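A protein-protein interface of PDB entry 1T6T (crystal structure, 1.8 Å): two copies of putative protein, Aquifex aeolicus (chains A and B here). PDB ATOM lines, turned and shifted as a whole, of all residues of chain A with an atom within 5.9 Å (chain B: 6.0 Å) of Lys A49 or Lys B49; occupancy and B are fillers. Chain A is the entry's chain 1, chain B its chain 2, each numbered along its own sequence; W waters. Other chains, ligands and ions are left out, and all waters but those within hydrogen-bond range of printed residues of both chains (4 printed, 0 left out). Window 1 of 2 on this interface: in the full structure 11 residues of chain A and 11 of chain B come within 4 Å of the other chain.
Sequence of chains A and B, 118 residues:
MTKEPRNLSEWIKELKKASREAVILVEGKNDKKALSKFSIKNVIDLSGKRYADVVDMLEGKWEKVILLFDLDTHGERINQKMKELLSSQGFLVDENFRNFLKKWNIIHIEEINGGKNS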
ATOM      1  N   ILE A  44      19.282 -15.865  19.253  1.00  0.00           N
ATOM      2  CA  ILE A  44      19.156 -14.416  19.171  1.00  0.00           C
ATOM      3  C   ILE A  44      18.115 -13.987  20.195  1.00  0.00           C
ATOM      4  O   ILE A  44      17.023 -14.563  20.249  1.00  0.00           O
ATOM      5  CB  ILE A  44      18.651 -13.943  17.794  1.00  0.00           C
ATOM      6  CG1 ILE A  44      19.671 -14.283  16.706  1.00  0.00           C
ATOM      7  CG2 ILE A  44      18.395 -12.432  17.832  1.00  0.00           C
ATOM      8  CD1 ILE A  44      19.205 -13.895  15.316  1.00  0.00           C
ATOM      9  N   ASP A  45      18.453 -12.996  21.016  1.00  0.00           N
ATOM     10  CA  ASP A  45      17.503 -12.486  21.999  1.00  0.00           C
ATOM     11  C   ASP A  45      16.847 -11.260  21.369  1.00  0.00           C
ATOM     12  O   ASP A  45      17.529 -10.385  20.830  1.00  0.00           O
ATOM     13  CB  ASP A  45      18.207 -12.151  23.329  1.00  0.00           C
ATOM     14  CG  ASP A  45      19.443 -11.282  23.156  1.00  0.00           C
ATOM     15  OD1 ASP A  45      20.221 -11.499  22.205  1.00  0.00           O
ATOM     16  OD2 ASP A  45      19.653 -10.388  24.001  1.00  0.00           O
ATOM     17  N   LEU A  46      15.521 -11.210  21.418  1.00  0.00           N
ATOM     18  CA  LEU A  46      14.776 -10.122  20.787  1.00  0.00           C
ATOM     19  C   LEU A  46      14.775  -8.778  21.505  1.00  0.00           C
ATOM     20  O   LEU A  46      14.783  -7.732  20.859  1.00  0.00           O
ATOM     21  CB  LEU A  46      13.330 -10.563  20.556  1.00  0.00           C
ATOM     22  CG  LEU A  46      12.428  -9.624  19.755  1.00  0.00           C
ATOM     23  CD1 LEU A  46      12.912  -9.546  18.317  1.00  0.00           C
ATOM     24  CD2 LEU A  46      10.997 -10.134  19.812  1.00  0.00           C
ATOM     25  N   SER A  47      14.756  -8.792  22.833  1.00  0.00           N
ATOM     26  CA  SER A  47      14.729  -7.541  23.577  1.00  0.00           C
ATOM     27  C   SER A  47      15.906  -6.659  23.184  1.00  0.00           C
ATOM     28  O   SER A  47      17.051  -7.106  23.185  1.00  0.00           O
ATOM     29  CB  SER A  47      14.756  -7.813  25.084  1.00  0.00           C
ATOM     30  OG  SER A  47      14.593  -6.608  25.810  1.00  0.00           O
ATOM     31  N   GLY A  48      15.616  -5.408  22.835  1.00  0.00           N
ATOM     32  CA  GLY A  48      16.668  -4.487  22.441  1.00  0.00           C
ATOM     33  C   GLY A  48      16.883  -4.430  20.938  1.00  0.00           C
ATOM     34  O   GLY A  48      17.774  -3.725  20.450  1.00  0.00           O
ATOM     35  N   LYS A  49      16.066  -5.174  20.198  1.00  0.00           N
ATOM     36  CA  LYS A  49      16.167  -5.203  18.743  1.00  0.00           C
ATOM     37  C   LYS A  49      14.827  -4.902  18.092  1.00  0.00           C
ATOM     38  O   LYS A  49      13.767  -5.163  18.664  1.00  0.00           O
ATOM     39  CB  LYS A  49      16.633  -6.586  18.260  1.00  0.00           C
ATOM     40  CG  LYS A  49      17.993  -7.019  18.786  1.00  0.00           C
ATOM     41  CD  LYS A  49      18.405  -8.362  18.189  1.00  0.00           C
ATOM     42  CE  LYS A  49      19.788  -8.786  18.657  1.00  0.00           C
ATOM     43  NZ  LYS A  49      19.830  -9.029  20.120  1.00  0.00           N
ATOM     44  N   ARG A  50      14.877  -4.339  16.891  1.00  0.00           N
ATOM     45  CA  ARG A  50      13.658  -4.070  16.143  1.00  0.00           C
ATOM     46  C   ARG A  50      13.332  -5.429  15.541  1.00  0.00           C
ATOM     47  O   ARG A  50      14.242  -6.208  15.261  1.00  0.00           O
ATOM     48  CB  ARG A  50      13.919  -3.071  15.021  1.00  0.00           C
ATOM     49  CG  ARG A  50      14.429  -1.717  15.485  1.00  0.00           C
ATOM     50  CD  ARG A  50      14.803  -0.859  14.291  1.00  0.00           C
ATOM     51  NE  ARG A  50      15.343   0.436  14.694  1.00  0.00           N
ATOM     52  CZ  ARG A  50      15.992   1.257  13.876  1.00  0.00           C
ATOM     53  NH1 ARG A  50      16.181   0.912  12.608  1.00  0.00           N
ATOM     54  NH2 ARG A  50      16.455   2.416  14.324  1.00  0.00           N
ATOM     55  N   TYR A  51      12.054  -5.728  15.345  1.00  0.00           N
ATOM     56  CA  TYR A  51      11.691  -7.019  14.775  1.00  0.00           C
ATOM     57  C   TYR A  51      12.423  -7.199  13.446  1.00  0.00           C
ATOM     58  O   TYR A  51      12.883  -8.295  13.122  1.00  0.00           O
ATOM     59  CB  TYR A  51      10.175  -7.112  14.560  1.00  0.00           C
ATOM     60  CG  TYR A  51       9.352  -6.843  15.802  1.00  0.00           C
ATOM     61  CD1 TYR A  51       9.720  -7.371  17.038  1.00  0.00           C
ATOM     62  CD2 TYR A  51       8.196  -6.069  15.736  1.00  0.00           C
ATOM     63  CE1 TYR A  51       8.958  -7.132  18.180  1.00  0.00           C
ATOM     64  CE2 TYR A  51       7.426  -5.826  16.868  1.00  0.00           C
ATOM     65  CZ  TYR A  51       7.813  -6.359  18.087  1.00  0.00           C
ATOM     66  OH  TYR A  51       7.059  -6.105  19.212  1.00  0.00           O
ATOM     67  N   ASP A  53      15.296  -6.138  12.712  1.00  0.00           N
ATOM     68  CA  ASP A  53      16.724  -6.376  12.910  1.00  0.00           C
ATOM     69  C   ASP A  53      16.986  -7.876  12.830  1.00  0.00           C
ATOM     70  O   ASP A  53      18.035  -8.305  12.351  1.00  0.00           O
ATOM     71  CB  ASP A  53      17.205  -5.865  14.277  1.00  0.00           C
ATOM     72  CG  ASP A  53      17.237  -4.349  14.366  1.00  0.00           C
ATOM     73  OD1 ASP A  53      17.267  -3.682  13.312  1.00  0.00           O
ATOM     74  OD2 ASP A  53      17.256  -3.827  15.502  1.00  0.00           O
ATOM     75  N   VAL A  54      16.030  -8.669  13.305  1.00  0.00           N
ATOM     76  CA  VAL A  54      16.166 -10.122  13.277  1.00  0.00           C
ATOM     77  C   VAL A  54      16.146 -10.606  11.827  1.00  0.00           C
ATOM     78  O   VAL A  54      16.918 -11.483  11.440  1.00  0.00           O
ATOM     79  CB  VAL A  54      15.021 -10.800  14.062  1.00  0.00           C
ATOM     80  CG1 VAL A  54      15.124 -12.319  13.954  1.00  0.00           C
ATOM     81  CG2 VAL A  54      15.082 -10.373  15.520  1.00  0.00           C
ATOM     82  N   MET A  57      19.435  -9.826  10.194  1.00  0.00           N
ATOM     83  CA  MET A  57      20.518 -10.674  10.693  1.00  0.00           C
ATOM     84  C   MET A  57      20.499 -12.070  10.071  1.00  0.00           C
ATOM     85  O   MET A  57      21.545 -12.687   9.888  1.00  0.00           O
ATOM     86  CB  MET A  57      20.420 -10.836  12.213  1.00  0.00           C
ATOM     87  CG  MET A  57      20.585  -9.561  13.009  1.00  0.00           C
ATOM     88  SD  MET A  57      20.181  -9.889  14.872  1.00  0.00           S
ATOM     89  CE  MET A  57      21.821 -10.778  15.386  1.00  0.00           C
ATOM     90  N   ILE B  44       5.495   5.576  24.964  1.00  0.00           N
ATOM     91  CA  ILE B  44       6.312   4.863  23.990  1.00  0.00           C
ATOM     92  C   ILE B  44       6.416   3.421  24.456  1.00  0.00           C
ATOM     93  O   ILE B  44       6.731   3.165  25.620  1.00  0.00           O
ATOM     94  CB  ILE B  44       7.754   5.424  23.894  1.00  0.00           C
ATOM     95  CG1 ILE B  44       7.734   6.838  23.310  1.00  0.00           C
ATOM     96  CG2 ILE B  44       8.616   4.501  23.016  1.00  0.00           C
ATOM     97  CD1 ILE B  44       9.109   7.473  23.233  1.00  0.00           C
ATOM     98  N   ASP B  45       6.130   2.486  23.558  1.00  0.00           N
ATOM     99  CA  ASP B  45       6.243   1.069  23.898  1.00  0.00           C
ATOM    100  C   ASP B  45       7.594   0.577  23.384  1.00  0.00           C
ATOM    101  O   ASP B  45       7.956   0.816  22.231  1.00  0.00           O
ATOM    102  CB  ASP B  45       5.072   0.268  23.303  1.00  0.00           C
ATOM    103  CG  ASP B  45       4.883   0.493  21.810  1.00  0.00           C
ATOM    104  OD1 ASP B  45       5.065   1.630  21.328  1.00  0.00           O
ATOM    105  OD2 ASP B  45       4.522  -0.480  21.118  1.00  0.00           O
ATOM    106  N   LEU B  46       8.339  -0.096  24.256  1.00  0.00           N
ATOM    107  CA  LEU B  46       9.681  -0.577  23.944  1.00  0.00           C
ATOM    108  C   LEU B  46       9.803  -1.783  23.007  1.00  0.00           C
ATOM    109  O   LEU B  46      10.720  -1.841  22.190  1.00  0.00           O
ATOM    110  CB  LEU B  46      10.417  -0.875  25.256  1.00  0.00           C
ATOM    111  CG  LEU B  46      11.929  -1.094  25.225  1.00  0.00           C
ATOM    112  CD1 LEU B  46      12.633   0.175  24.757  1.00  0.00           C
ATOM    113  CD2 LEU B  46      12.405  -1.479  26.620  1.00  0.00           C
ATOM    114  N   SER B  47       8.900  -2.750  23.121  1.00  0.00           N
ATOM    115  CA  SER B  47       8.993  -3.929  22.264  1.00  0.00           C
ATOM    116  C   SER B  47       9.023  -3.530  20.795  1.00  0.00           C
ATOM    117  O   SER B  47       8.209  -2.726  20.341  1.00  0.00           O
ATOM    118  CB  SER B  47       7.819  -4.878  22.518  1.00  0.00           C
ATOM    119  OG  SER B  47       7.965  -6.060  21.743  1.00  0.00           O
ATOM    120  N   GLY B  48       9.975  -4.089  20.055  1.00  0.00           N
ATOM    121  CA  GLY B  48      10.091  -3.764  18.647  1.00  0.00           C
ATOM    122  C   GLY B  48      11.021  -2.588  18.404  1.00  0.00           C
ATOM    123  O   GLY B  48      11.177  -2.136  17.269  1.00  0.00           O
ATOM    124  N   LYS B  49      11.635  -2.080  19.470  1.00  0.00           N
ATOM    125  CA  LYS B  49      12.566  -0.963  19.349  1.00  0.00           C
ATOM    126  C   LYS B  49      13.906  -1.270  20.017  1.00  0.00           C
ATOM    127  O   LYS B  49      13.974  -2.060  20.959  1.00  0.00           O
ATOM    128  CB  LYS B  49      11.984   0.303  19.999  1.00  0.00           C
ATOM    129  CG  LYS B  49      10.637   0.761  19.444  1.00  0.00           C
ATOM    130  CD  LYS B  49      10.215   2.088  20.079  1.00  0.00           C
ATOM    131  CE  LYS B  49       8.916   2.625  19.483  1.00  0.00           C
ATOM    132  NZ  LYS B  49       7.746   1.743  19.744  1.00  0.00           N
ATOM    133  N   ARG B  50      14.977  -0.663  19.512  1.00  0.00           N
ATOM    134  CA  ARG B  50      16.292  -0.824  20.130  1.00  0.00           C
ATOM    135  C   ARG B  50      16.220   0.149  21.302  1.00  0.00           C
ATOM    136  O   ARG B  50      15.480   1.131  21.237  1.00  0.00           O
ATOM    137  CB  ARG B  50      17.401  -0.381  19.176  1.00  0.00           C
ATOM    138  CG  ARG B  50      17.438  -1.149  17.871  1.00  0.00           C
ATOM    139  CD  ARG B  50      18.337  -0.457  16.868  1.00  0.00           C
ATOM    140  NE  ARG B  50      18.360  -1.153  15.585  1.00  0.00           N
ATOM    141  CZ  ARG B  50      18.989  -0.701  14.505  1.00  0.00           C
ATOM    142  NH1 ARG B  50      19.650   0.450  14.554  1.00  0.00           N
ATOM    143  NH2 ARG B  50      18.961  -1.399  13.379  1.00  0.00           N
ATOM    144  N   TYR B  51      16.965  -0.109  22.371  1.00  0.00           N
ATOM    145  CA  TYR B  51      16.922   0.797  23.507  1.00  0.00           C
ATOM    146  C   TYR B  51      17.345   2.184  23.032  1.00  0.00           C
ATOM    147  O   TYR B  51      16.779   3.194  23.453  1.00  0.00           O
ATOM    148  CB  TYR B  51      17.849   0.316  24.629  1.00  0.00           C
ATOM    149  CG  TYR B  51      17.606  -1.115  25.059  1.00  0.00           C
ATOM    150  CD1 TYR B  51      16.314  -1.603  25.231  1.00  0.00           C
ATOM    151  CD2 TYR B  51      18.674  -1.981  25.297  1.00  0.00           C
ATOM    152  CE1 TYR B  51      16.087  -2.918  25.627  1.00  0.00           C
ATOM    153  CE2 TYR B  51      18.459  -3.297  25.694  1.00  0.00           C
ATOM    154  CZ  TYR B  51      17.163  -3.760  25.857  1.00  0.00           C
ATOM    155  OH  TYR B  51      16.944  -5.063  26.241  1.00  0.00           O
ATOM    156  N   ASP B  53      16.779   3.505  20.248  1.00  0.00           N
ATOM    157  CA  ASP B  53      15.719   4.147  19.471  1.00  0.00           C
ATOM    158  C   ASP B  53      14.921   5.087  20.373  1.00  0.00           C
ATOM    159  O   ASP B  53      14.483   6.153  19.939  1.00  0.00           O
ATOM    160  CB  ASP B  53      14.758   3.117  18.854  1.00  0.00           C
ATOM    161  CG  ASP B  53      15.384   2.319  17.716  1.00  0.00           C
ATOM    162  OD1 ASP B  53      16.364   2.794  17.104  1.00  0.00           O
ATOM    163  OD2 ASP B  53      14.875   1.216  17.416  1.00  0.00           O
ATOM    164  N   VAL B  54      14.721   4.686  21.625  1.00  0.00           N
ATOM    165  CA  VAL B  54      13.981   5.509  22.576  1.00  0.00           C
ATOM    166  C   VAL B  54      14.766   6.788  22.852  1.00  0.00           C
ATOM    167  O   VAL B  54      14.205   7.881  22.900  1.00  0.00           O
ATOM    168  CB  VAL B  54      13.753   4.750  23.904  1.00  0.00           C
ATOM    169  CG1 VAL B  54      13.089   5.663  24.930  1.00  0.00           C
ATOM    170  CG2 VAL B  54      12.891   3.526  23.647  1.00  0.00           C
ATOM    171  N   MET B  57      14.509   9.128  19.919  1.00  0.00           N
ATOM    172  CA  MET B  57      13.160   9.686  19.817  1.00  0.00           C
ATOM    173  C   MET B  57      12.934  10.836  20.791  1.00  0.00           C
ATOM    174  O   MET B  57      12.191  11.772  20.496  1.00  0.00           O
ATOM    175  CB  MET B  57      12.116   8.608  20.114  1.00  0.00           C
ATOM    176  CG  MET B  57      11.955   7.552  19.050  1.00  0.00           C
ATOM    177  SD  MET B  57      10.828   6.114  19.706  1.00  0.00           S
ATOM    178  CE  MET B  57       9.099   6.960  19.510  1.00  0.00           C
HETATM  179  O   HOH W   1      10.113  -3.480  15.216  1.00  0.00           O
HETATM  180  O   HOH W   2      13.050  -4.014  22.657  1.00  0.00           O
HETATM  181  O   HOH W   3      12.159  -5.868  20.703  1.00  0.00           O
HETATM  182  O   HOH W   4      19.010  -2.185  22.159  1.00  0.00           O
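The side-chain hydroxyl (OG) of Ser A47 lies within hydrogen-bond range of the side-chain hydroxyl (OH) of Tyr B51 (2.8 Å).
The side-chain carboxylate of Asp B53 lies within salt-bridge range of the guanidinium group of Arg A50, 2.8 Å away.
The side-chain hydroxyl of Tyr A51 is in hydrogen-bond range of the side-chain hydroxyl of Ser B47.
The side-chain carboxylate (OD1) of Asp A53 is in salt-bridge range of the guanidinium group (NH2) of Arg B50, 2.8 Å away.
The side-chain carboxylate of Asp A45 is in salt-bridge range of the side-chain amino group of Lys A49 (3.3 Å).
The backbone NH (N) of Arg A50 lies within hydrogen-bond range of the side-chain carboxylate (OD2) of Asp A53, 2.8 Å away.
OD1 of Asp B45 is in salt-bridge range of NZ of Lys B49, 3.1 Å away.
The side-chain carboxylate of Asp B53 lies within hydrogen-bond range of the backbone NH of Arg B50, 2.8 Å away.
Gly A48 touches Lys B49 (C to O, 3.8 Å).
Arg B50 touches Gly A48.
Tyr B51 touches Gly A48 (CZ to CA, 3.5 Å).
Lys A49 touches Gly B48.
N of Lys A49 touches O of Lys B49, at 3.8 Å.
O of Gly B48 touches CA of Arg A50, 3.3 Å away.
Arg A50 touches Arg B50.
Tyr A51 touches Gly B48 (CZ to CA, 3.5 Å).
Of chain B, only Gly B48 and Lys B49 come within 4 Å of Lys A49.
Printed residues of chain A within 4 Å of Lys B49: Gly A48 and Lys A49.
Printed residues of chain A within 4 Å of Asp B53: Arg A50.
Printed residues of chain A within 4 Å of Gly B48: Lys A49, Arg A50 and Tyr A51.
Of the printed residues of chain B, Gly A48 touches Lys B49 (3.8 Å), Arg B50 (3.3 Å) and Tyr B51 (3.5 Å).
Asp B45 touches none of the printed residues of chain A.
The nearest printed residue of chain A that does not touch Asp B53 is Asp A53 (5.9 Å).
Of the 11 printed residues of chain A, 6 touch a printed residue of chain B.
Printed residues of chain A that touch a printed residue of chain B: Ser A47, Gly A48, Lys A49, Arg A50, Tyr A51 and Asp A53.
Of the 11 printed residues of chain B, 6 touch a printed residue of chain A.
Printed residues of chain B that touch a printed residue of chain A: Ser B47, Gly B48, Lys B49, Arg B50, Tyr B51 and Asp B53.
Hydrophobic or aromatic side chains of chain B within 4 Å of the printed part of chain A: Tyr B51.
Among the printed residues, 12 pairs touch across the chains.
Ser A47 touches Tyr B51, and with the chains exchanged Tyr A51 touches Ser B47.
Gly A48 touches Lys B49, and with the chains exchanged Lys A49 touches Gly B48.
Lys A49 touches its own counterpart, Lys B49.
Arg A50 touches Asp B53, and with the chains exchanged Asp A53 touches Arg B50.
Of the 12 pairs that touch across the chains among the printed residues, 12 have their exchanged pair printed and touching as well.
Water W4 lies within hydrogen-bond range of O of Gly A48 and N of Tyr B51.
Water W1 lies within hydrogen-bond range of O of Gly B48 (2.7 Å) and N of Tyr A51 (3.0 Å).
Water W3 lies within hydrogen-bond range of the backbone carbonyl oxygen (O) of Lys A49 (2.7 Å), the backbone NH (N) of Gly B48 (2.9 Å) and the backbone carbonyl oxygen (O) of Leu A46 (3.2 Å).
Water W2 lies within hydrogen-bond range of the backbone carbonyl oxygen of Lys B49 (2.7 Å), the backbone NH of Gly A48 (2.9 Å) and the backbone carbonyl oxygen of Leu B46 (3.2 Å).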
